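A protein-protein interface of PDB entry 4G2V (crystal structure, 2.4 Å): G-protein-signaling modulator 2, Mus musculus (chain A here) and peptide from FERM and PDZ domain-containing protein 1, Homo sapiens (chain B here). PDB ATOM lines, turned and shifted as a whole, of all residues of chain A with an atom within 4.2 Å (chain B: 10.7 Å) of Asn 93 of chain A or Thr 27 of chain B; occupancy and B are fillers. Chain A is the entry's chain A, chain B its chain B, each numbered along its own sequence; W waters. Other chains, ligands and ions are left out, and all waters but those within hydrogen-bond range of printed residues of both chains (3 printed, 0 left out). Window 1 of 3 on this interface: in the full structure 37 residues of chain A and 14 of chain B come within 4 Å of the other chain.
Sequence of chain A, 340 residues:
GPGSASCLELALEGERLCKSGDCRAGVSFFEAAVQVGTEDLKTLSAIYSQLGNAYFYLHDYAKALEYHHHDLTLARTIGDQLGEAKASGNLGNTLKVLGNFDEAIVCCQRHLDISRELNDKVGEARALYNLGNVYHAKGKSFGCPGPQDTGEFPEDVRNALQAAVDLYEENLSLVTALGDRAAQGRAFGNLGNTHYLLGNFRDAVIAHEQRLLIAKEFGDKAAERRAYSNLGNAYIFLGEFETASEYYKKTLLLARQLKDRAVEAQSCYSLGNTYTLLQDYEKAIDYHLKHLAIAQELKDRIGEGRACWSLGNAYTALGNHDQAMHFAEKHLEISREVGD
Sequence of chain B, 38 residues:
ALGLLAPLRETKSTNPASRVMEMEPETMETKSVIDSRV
The backbone carbonyl oxygen (O) of Asn 90 of chain A sits at hydrogen-bond distance from the side-chain hydroxyl (OG1) of Thr 94 of chain A (2.9 Å).
The side-chain amide oxygen of Asn 93 of chain A is in hydrogen-bond range of the side-chain sulfur of Cys 108 of chain A (3.7 Å).
ND2 of Asn 93 of chain A is in hydrogen-bond range of OD1 of Asn 130 of chain A.
The side-chain amide nitrogen (ND2) of Asn 130 of chain A sits at hydrogen-bond distance from the backbone carbonyl oxygen (O) of Arg 126 of chain A, at 3.2 Å.
Water W3 bridges OG1 of Thr 27 of chain B (2.5 Å) and O of Arg 126 of chain A (3.0 Å).
Water W2 lies within hydrogen-bond range of OE2 of Glu 29 of chain B, OG1 of Thr 27 of chain B and ND2 of Asn 130 of chain A.
Water W1 lies within hydrogen-bond range of the side-chain amide oxygen (OD1) of Asn 90 of chain A (2.9 Å), the side-chain amide nitrogen (ND2) of Asn 93 of chain A (3.1 Å), the backbone NH (N) of Glu 29 of chain B (3.4 Å) and the backbone carbonyl oxygen (O) of Gly 89 of chain A (3.5 Å).
No residue of chain B comes within 4 Å of Gly 89 of chain A.
Leu 91 of chain A touches none of the printed residues of chain B.
Asn 93 of chain A touches just these residues of chain B: Thr 27 and Met 28.
Thr 94 of chain A touches none of the printed residues of chain B.
Of chain B, only Glu 26 (2.9 Å) comes within 4 Å of Lys 96 of chain A.
Val 97 of chain A touches one residue of chain B.
Of chain B, only Thr 27, Met 28 and Glu 29 come within 4 Å of Arg 126 of chain A.
Of chain B, only Thr 27 comes within 4 Å of Asn 130 of chain A.
Printed residues of chain A within 4 Å of Glu 24 of chain B: Arg 186.
Thr 27 of chain B touches just these residues of chain A: Asn 93 (2.7 Å), Arg 126 (3.5 Å), Asn 130 (3.1 Å) and Arg 186 (3.5 Å).
Printed residues of chain A within 4 Å of Met 28 of chain B: Phe 56, Asn 90, Asn 93 and Arg 126.
The nearest printed residue of chain A that does not touch Thr 27 of chain B is Asn 90 of chain A (5.0 Å).
The nearest printed residue of chain B that does not touch Arg 186 of chain A is Pro 25 of chain B (4.03 Å).
Of the 14 printed residues of chain A, 8 touch a printed residue of chain B.
Of the 8 printed residues of chain B, 5 touch a printed residue of chain A.
Hydrophobic or aromatic side chains of chain B that line the printed part of chain A: Met 28.
Among the printed residues, 13 pairs touch across the chains.
OD1 of Asn 90 of chain A lies within hydrogen-bond range of N of Glu 29 of chain B (2.7 Å).
The backbone carbonyl oxygen (O) of Thr 27 of chain B lies within hydrogen-bond range of the side-chain amide nitrogen (ND2) of Asn 93 of chain A, at 2.7 Å.
SD of Met 28 of chain B lies within hydrogen-bond range of ND2 of Asn 93 of chain A.
OE2 of Glu 26 of chain B is in salt-bridge range of NZ of Lys 96 of chain A (2.9 Å).
NH2 of Arg 126 of chain A sits at hydrogen-bond distance from O of Met 28 of chain B, 3.0 Å away.
The guanidinium group (NE) of Arg 126 of chain A lies within salt-bridge range of the side-chain carboxylate (OE2) of Glu 29 of chain B, at 2.7 Å.
The side-chain amide oxygen of Asn 130 of chain A lies within hydrogen-bond range of the side-chain hydroxyl of Thr 27 of chain B, 3.1 Å away.
Among the printed residues, pairs that only touch across the chains: Arg 186 of chain A with Glu 24 of chain B (3.3 Å), Asn 90 of chain A with Met 28 of chain B (3.4 Å), Arg 126 of chain A with Thr 27 of chain B (3.5 Å), Arg 186 of chain A with Thr 27 of chain B (3.5 Å), Val 97 of chain A with Glu 26 of chain B (3.9 Å) and Phe 56 of chain A with Met 28 of chain B (3.998 Å).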
ATOM      1  N   PHE A  56      -3.602  18.210  -4.036  1.00  0.00           N
ATOM      2  CA  PHE A  56      -2.368  17.931  -4.757  1.00  0.00           C
ATOM      3  C   PHE A  56      -2.348  16.471  -5.201  1.00  0.00           C
ATOM      4  O   PHE A  56      -2.004  16.160  -6.342  1.00  0.00           O
ATOM      5  CB  PHE A  56      -1.155  18.230  -3.876  1.00  0.00           C
ATOM      6  CG  PHE A  56       0.164  17.924  -4.530  1.00  0.00           C
ATOM      7  CD1 PHE A  56       0.653  16.624  -4.567  1.00  0.00           C
ATOM      8  CD2 PHE A  56       0.926  18.938  -5.094  1.00  0.00           C
ATOM      9  CE1 PHE A  56       1.868  16.337  -5.167  1.00  0.00           C
ATOM     10  CE2 PHE A  56       2.145  18.663  -5.692  1.00  0.00           C
ATOM     11  CZ  PHE A  56       2.617  17.355  -5.731  1.00  0.00           C
ATOM     12  N   GLY A  89       7.423  24.579   1.810  1.00  0.00           N
ATOM     13  CA  GLY A  89       7.799  23.412   1.032  1.00  0.00           C
ATOM     14  C   GLY A  89       6.645  22.869   0.204  1.00  0.00           C
ATOM     15  O   GLY A  89       6.813  22.520  -0.962  1.00  0.00           O
ATOM     16  N   ASN A  90       5.464  22.791   0.807  1.00  0.00           N
ATOM     17  CA  ASN A  90       4.282  22.331   0.086  1.00  0.00           C
ATOM     18  C   ASN A  90       3.897  23.257  -1.071  1.00  0.00           C
ATOM     19  O   ASN A  90       3.541  22.802  -2.162  1.00  0.00           O
ATOM     20  CB  ASN A  90       3.110  22.143   1.050  1.00  0.00           C
ATOM     21  CG  ASN A  90       3.342  21.006   2.037  1.00  0.00           C
ATOM     22  OD1 ASN A  90       4.059  20.050   1.741  1.00  0.00           O
ATOM     23  ND2 ASN A  90       2.737  21.108   3.213  1.00  0.00           N
ATOM     24  N   LEU A  91       3.978  24.561  -0.832  1.00  0.00           N
ATOM     25  CA  LEU A  91       3.729  25.531  -1.887  1.00  0.00           C
ATOM     26  C   LEU A  91       4.780  25.367  -2.976  1.00  0.00           C
ATOM     27  O   LEU A  91       4.473  25.435  -4.167  1.00  0.00           O
ATOM     28  CB  LEU A  91       3.754  26.950  -1.326  1.00  0.00           C
ATOM     29  CG  LEU A  91       3.372  28.081  -2.277  1.00  0.00           C
ATOM     30  CD1 LEU A  91       1.953  27.900  -2.811  1.00  0.00           C
ATOM     31  CD2 LEU A  91       3.522  29.415  -1.568  1.00  0.00           C
ATOM     32  N   GLY A  92       6.020  25.141  -2.552  1.00  0.00           N
ATOM     33  CA  GLY A  92       7.126  24.948  -3.472  1.00  0.00           C
ATOM     34  C   GLY A  92       6.875  23.805  -4.435  1.00  0.00           C
ATOM     35  O   GLY A  92       6.947  23.975  -5.654  1.00  0.00           O
ATOM     36  N   ASN A  93       6.568  22.637  -3.884  1.00  0.00           N
ATOM     37  CA  ASN A  93       6.306  21.454  -4.698  1.00  0.00           C
ATOM     38  C   ASN A  93       5.133  21.658  -5.656  1.00  0.00           C
ATOM     39  O   ASN A  93       5.144  21.173  -6.790  1.00  0.00           O
ATOM     40  CB  ASN A  93       6.077  20.229  -3.804  1.00  0.00           C
ATOM     41  CG  ASN A  93       7.325  19.847  -3.016  1.00  0.00           C
ATOM     42  OD1 ASN A  93       8.437  20.256  -3.361  1.00  0.00           O
ATOM     43  ND2 ASN A  93       7.149  19.055  -1.964  1.00  0.00           N
ATOM     44  N   THR A  94       4.123  22.384  -5.197  1.00  0.00           N
ATOM     45  CA  THR A  94       2.942  22.624  -6.014  1.00  0.00           C
ATOM     46  C   THR A  94       3.304  23.523  -7.194  1.00  0.00           C
ATOM     47  O   THR A  94       2.923  23.247  -8.332  1.00  0.00           O
ATOM     48  CB  THR A  94       1.802  23.236  -5.186  1.00  0.00           C
ATOM     49  OG1 THR A  94       1.485  22.361  -4.094  1.00  0.00           O
ATOM     50  CG2 THR A  94       0.561  23.444  -6.043  1.00  0.00           C
ATOM     51  N   LEU A  95       4.065  24.579  -6.914  1.00  0.00           N
ATOM     52  CA  LEU A  95       4.541  25.495  -7.952  1.00  0.00           C
ATOM     53  C   LEU A  95       5.387  24.776  -9.000  1.00  0.00           C
ATOM     54  O   LEU A  95       5.371  25.137 -10.179  1.00  0.00           O
ATOM     55  CB  LEU A  95       5.336  26.645  -7.330  1.00  0.00           C
ATOM     56  CG  LEU A  95       4.496  27.680  -6.573  1.00  0.00           C
ATOM     57  CD1 LEU A  95       5.326  28.446  -5.538  1.00  0.00           C
ATOM     58  CD2 LEU A  95       3.785  28.638  -7.541  1.00  0.00           C
ATOM     59  N   LYS A  96       6.117  23.754  -8.561  1.00  0.00           N
ATOM     60  CA  LYS A  96       6.951  22.968  -9.464  1.00  0.00           C
ATOM     61  C   LYS A  96       6.092  22.232 -10.482  1.00  0.00           C
ATOM     62  O   LYS A  96       6.375  22.252 -11.679  1.00  0.00           O
ATOM     63  CB  LYS A  96       7.796  21.961  -8.683  1.00  0.00           C
ATOM     64  CG  LYS A  96       8.803  21.212  -9.544  1.00  0.00           C
ATOM     65  CD  LYS A  96       9.137  19.853  -8.958  1.00  0.00           C
ATOM     66  CE  LYS A  96       7.870  19.030  -8.781  1.00  0.00           C
ATOM     67  NZ  LYS A  96       8.159  17.637  -8.381  1.00  0.00           N
ATOM     68  N   VAL A  97       5.039  21.581 -10.000  1.00  0.00           N
ATOM     69  CA  VAL A  97       4.120  20.874 -10.882  1.00  0.00           C
ATOM     70  C   VAL A  97       3.473  21.835 -11.876  1.00  0.00           C
ATOM     71  O   VAL A  97       3.271  21.492 -13.040  1.00  0.00           O
ATOM     72  CB  VAL A  97       3.014  20.149 -10.085  1.00  0.00           C
ATOM     73  CG1 VAL A  97       1.962  19.583 -11.029  1.00  0.00           C
ATOM     74  CG2 VAL A  97       3.612  19.048  -9.215  1.00  0.00           C
ATOM     75  N   CYS A 108      10.969  26.321  -1.714  1.00  0.00           N
ATOM     76  CA  CYS A 108      11.658  25.154  -1.193  1.00  0.00           C
ATOM     77  C   CYS A 108      12.929  25.582  -0.455  1.00  0.00           C
ATOM     78  O   CYS A 108      13.311  24.969   0.541  1.00  0.00           O
ATOM     79  CB  CYS A 108      11.952  24.138  -2.307  1.00  0.00           C
ATOM     80  SG  CYS A 108      10.465  23.329  -2.993  1.00  0.00           S
ATOM     81  N   ARG A 126      14.620  16.802   3.799  1.00  0.00           N
ATOM     82  CA  ARG A 126      13.449  16.735   2.933  1.00  0.00           C
ATOM     83  C   ARG A 126      13.388  17.934   1.997  1.00  0.00           C
ATOM     84  O   ARG A 126      13.050  17.800   0.821  1.00  0.00           O
ATOM     85  CB  ARG A 126      12.164  16.594   3.754  1.00  0.00           C
ATOM     86  CG  ARG A 126      11.971  15.189   4.312  1.00  0.00           C
ATOM     87  CD  ARG A 126      10.913  15.113   5.399  1.00  0.00           C
ATOM     88  NE  ARG A 126       9.552  15.119   4.867  1.00  0.00           N
ATOM     89  CZ  ARG A 126       8.911  14.032   4.444  1.00  0.00           C
ATOM     90  NH1 ARG A 126       9.513  12.849   4.472  1.00  0.00           N
ATOM     91  NH2 ARG A 126       7.669  14.127   3.982  1.00  0.00           N
ATOM     92  N   ASN A 130      13.252  17.983  -2.247  1.00  0.00           N
ATOM     93  CA  ASN A 130      12.285  18.802  -2.977  1.00  0.00           C
ATOM     94  C   ASN A 130      12.956  19.827  -3.890  1.00  0.00           C
ATOM     95  O   ASN A 130      12.535  20.031  -5.034  1.00  0.00           O
ATOM     96  CB  ASN A 130      11.361  19.538  -2.009  1.00  0.00           C
ATOM     97  CG  ASN A 130      10.492  18.600  -1.194  1.00  0.00           C
ATOM     98  OD1 ASN A 130      10.090  17.535  -1.661  1.00  0.00           O
ATOM     99  ND2 ASN A 130      10.189  19.004   0.033  1.00  0.00           N
ATOM    100  N   ARG A 186      14.395   7.369  -2.550  1.00  0.00           N
ATOM    101  CA  ARG A 186      13.875   8.447  -3.387  1.00  0.00           C
ATOM    102  C   ARG A 186      14.990   9.235  -4.071  1.00  0.00           C
ATOM    103  O   ARG A 186      14.942   9.475  -5.279  1.00  0.00           O
ATOM    104  CB  ARG A 186      13.006   9.396  -2.565  1.00  0.00           C
ATOM    105  CG  ARG A 186      11.673   8.800  -2.170  1.00  0.00           C
ATOM    106  CD  ARG A 186      10.798   9.820  -1.474  1.00  0.00           C
ATOM    107  NE  ARG A 186      11.371  10.272  -0.210  1.00  0.00           N
ATOM    108  CZ  ARG A 186      11.049   9.771   0.978  1.00  0.00           C
ATOM    109  NH1 ARG A 186      10.158   8.792   1.069  1.00  0.00           N
ATOM    110  NH2 ARG A 186      11.613  10.254   2.080  1.00  0.00           N
ATOM    111  N   MET B  23      10.452   8.305 -12.353  1.00  0.00           N
ATOM    112  CA  MET B  23      10.808   9.163 -11.231  1.00  0.00           C
ATOM    113  C   MET B  23      10.310   8.632  -9.891  1.00  0.00           C
ATOM    114  O   MET B  23       9.338   7.877  -9.824  1.00  0.00           O
ATOM    115  CB  MET B  23      10.280  10.583 -11.450  1.00  0.00           C
ATOM    116  CG  MET B  23      10.740  11.218 -12.754  1.00  0.00           C
ATOM    117  SD  MET B  23      12.528  11.447 -12.840  1.00  0.00           S
ATOM    118  CE  MET B  23      12.770  12.673 -11.558  1.00  0.00           C
ATOM    119  N   GLU B  24      10.996   9.036  -8.828  1.00  0.00           N
ATOM    120  CA  GLU B  24      10.480   8.891  -7.476  1.00  0.00           C
ATOM    121  C   GLU B  24       9.527  10.049  -7.165  1.00  0.00           C
ATOM    122  O   GLU B  24       9.693  11.159  -7.679  1.00  0.00           O
ATOM    123  CB  GLU B  24      11.634   8.849  -6.474  1.00  0.00           C
ATOM    124  CG  GLU B  24      12.585   7.690  -6.725  1.00  0.00           C
ATOM    125  CD  GLU B  24      11.867   6.352  -6.699  1.00  0.00           C
ATOM    126  OE1 GLU B  24      11.154   6.088  -5.709  1.00  0.00           O
ATOM    127  OE2 GLU B  24      11.995   5.574  -7.669  1.00  0.00           O
ATOM    128  N   PRO B  25       8.522   9.794  -6.318  1.00  0.00           N
ATOM    129  CA  PRO B  25       7.477  10.780  -6.026  1.00  0.00           C
ATOM    130  C   PRO B  25       7.968  11.922  -5.141  1.00  0.00           C
ATOM    131  O   PRO B  25       9.012  11.813  -4.491  1.00  0.00           O
ATOM    132  CB  PRO B  25       6.435   9.955  -5.271  1.00  0.00           C
ATOM    133  CG  PRO B  25       7.243   8.900  -4.580  1.00  0.00           C
ATOM    134  CD  PRO B  25       8.352   8.556  -5.537  1.00  0.00           C
ATOM    135  N   GLU B  26       7.214  13.016  -5.128  1.00  0.00           N
ATOM    136  CA  GLU B  26       7.472  14.114  -4.206  1.00  0.00           C
ATOM    137  C   GLU B  26       7.149  13.681  -2.780  1.00  0.00           C
ATOM    138  O   GLU B  26       6.441  12.701  -2.560  1.00  0.00           O
ATOM    139  CB  GLU B  26       6.620  15.343  -4.550  1.00  0.00           C
ATOM    140  CG  GLU B  26       6.867  15.950  -5.925  1.00  0.00           C
ATOM    141  CD  GLU B  26       5.940  15.388  -6.983  1.00  0.00           C
ATOM    142  OE1 GLU B  26       5.335  14.322  -6.735  1.00  0.00           O
ATOM    143  OE2 GLU B  26       5.811  16.014  -8.057  1.00  0.00           O
ATOM    144  N   THR B  27       7.675  14.427  -1.819  1.00  0.00           N
ATOM    145  CA  THR B  27       7.204  14.345  -0.448  1.00  0.00           C
ATOM    146  C   THR B  27       6.431  15.628  -0.156  1.00  0.00           C
ATOM    147  O   THR B  27       6.651  16.660  -0.787  1.00  0.00           O
ATOM    148  CB  THR B  27       8.368  14.219   0.555  1.00  0.00           C
ATOM    149  OG1 THR B  27       9.252  15.332   0.397  1.00  0.00           O
ATOM    150  CG2 THR B  27       9.142  12.924   0.327  1.00  0.00           C
ATOM    151  N   MET B  28       5.486  15.554   0.767  1.00  0.00           N
ATOM    152  CA  MET B  28       4.829  16.760   1.245  1.00  0.00           C
ATOM    153  C   MET B  28       4.987  16.813   2.759  1.00  0.00           C
ATOM    154  O   MET B  28       5.230  15.794   3.396  1.00  0.00           O
ATOM    155  CB  MET B  28       3.353  16.780   0.829  1.00  0.00           C
ATOM    156  CG  MET B  28       3.131  16.661  -0.689  1.00  0.00           C
ATOM    157  SD  MET B  28       3.741  18.059  -1.687  1.00  0.00           S
ATOM    158  CE  MET B  28       2.451  19.284  -1.414  1.00  0.00           C
ATOM    159  N   GLU B  29       4.893  18.004   3.334  1.00  0.00           N
ATOM    160  CA  GLU B  29       4.893  18.127   4.780  1.00  0.00           C
ATOM    161  C   GLU B  29       3.455  18.071   5.272  1.00  0.00           C
ATOM    162  O   GLU B  29       2.552  18.636   4.652  1.00  0.00           O
ATOM    163  CB  GLU B  29       5.580  19.420   5.218  1.00  0.00           C
ATOM    164  CG  GLU B  29       7.041  19.487   4.803  1.00  0.00           C
ATOM    165  CD  GLU B  29       7.847  18.325   5.356  1.00  0.00           C
ATOM    166  OE1 GLU B  29       7.839  18.136   6.588  1.00  0.00           O
ATOM    167  OE2 GLU B  29       8.479  17.597   4.562  1.00  0.00           O
ATOM    168  N   THR B  30       3.242  17.370   6.377  1.00  0.00           N
ATOM    169  CA  THR B  30       1.892  17.158   6.874  1.00  0.00           C
ATOM    170  C   THR B  30       1.669  17.797   8.237  1.00  0.00           C
ATOM    171  O   THR B  30       2.584  17.901   9.059  1.00  0.00           O
ATOM    172  CB  THR B  30       1.552  15.661   6.939  1.00  0.00           C
ATOM    173  OG1 THR B  30       2.493  14.995   7.787  1.00  0.00           O
ATOM    174  CG2 THR B  30       1.621  15.047   5.549  1.00  0.00           C
HETATM  175  O   HOH W   1       6.841  19.689   1.095  1.00  0.00           O
HETATM  176  O   HOH W   2       8.410  17.525   1.925  1.00  0.00           O
HETATM  177  O   HOH W   3      11.706  15.076   0.757  1.00  0.00           O
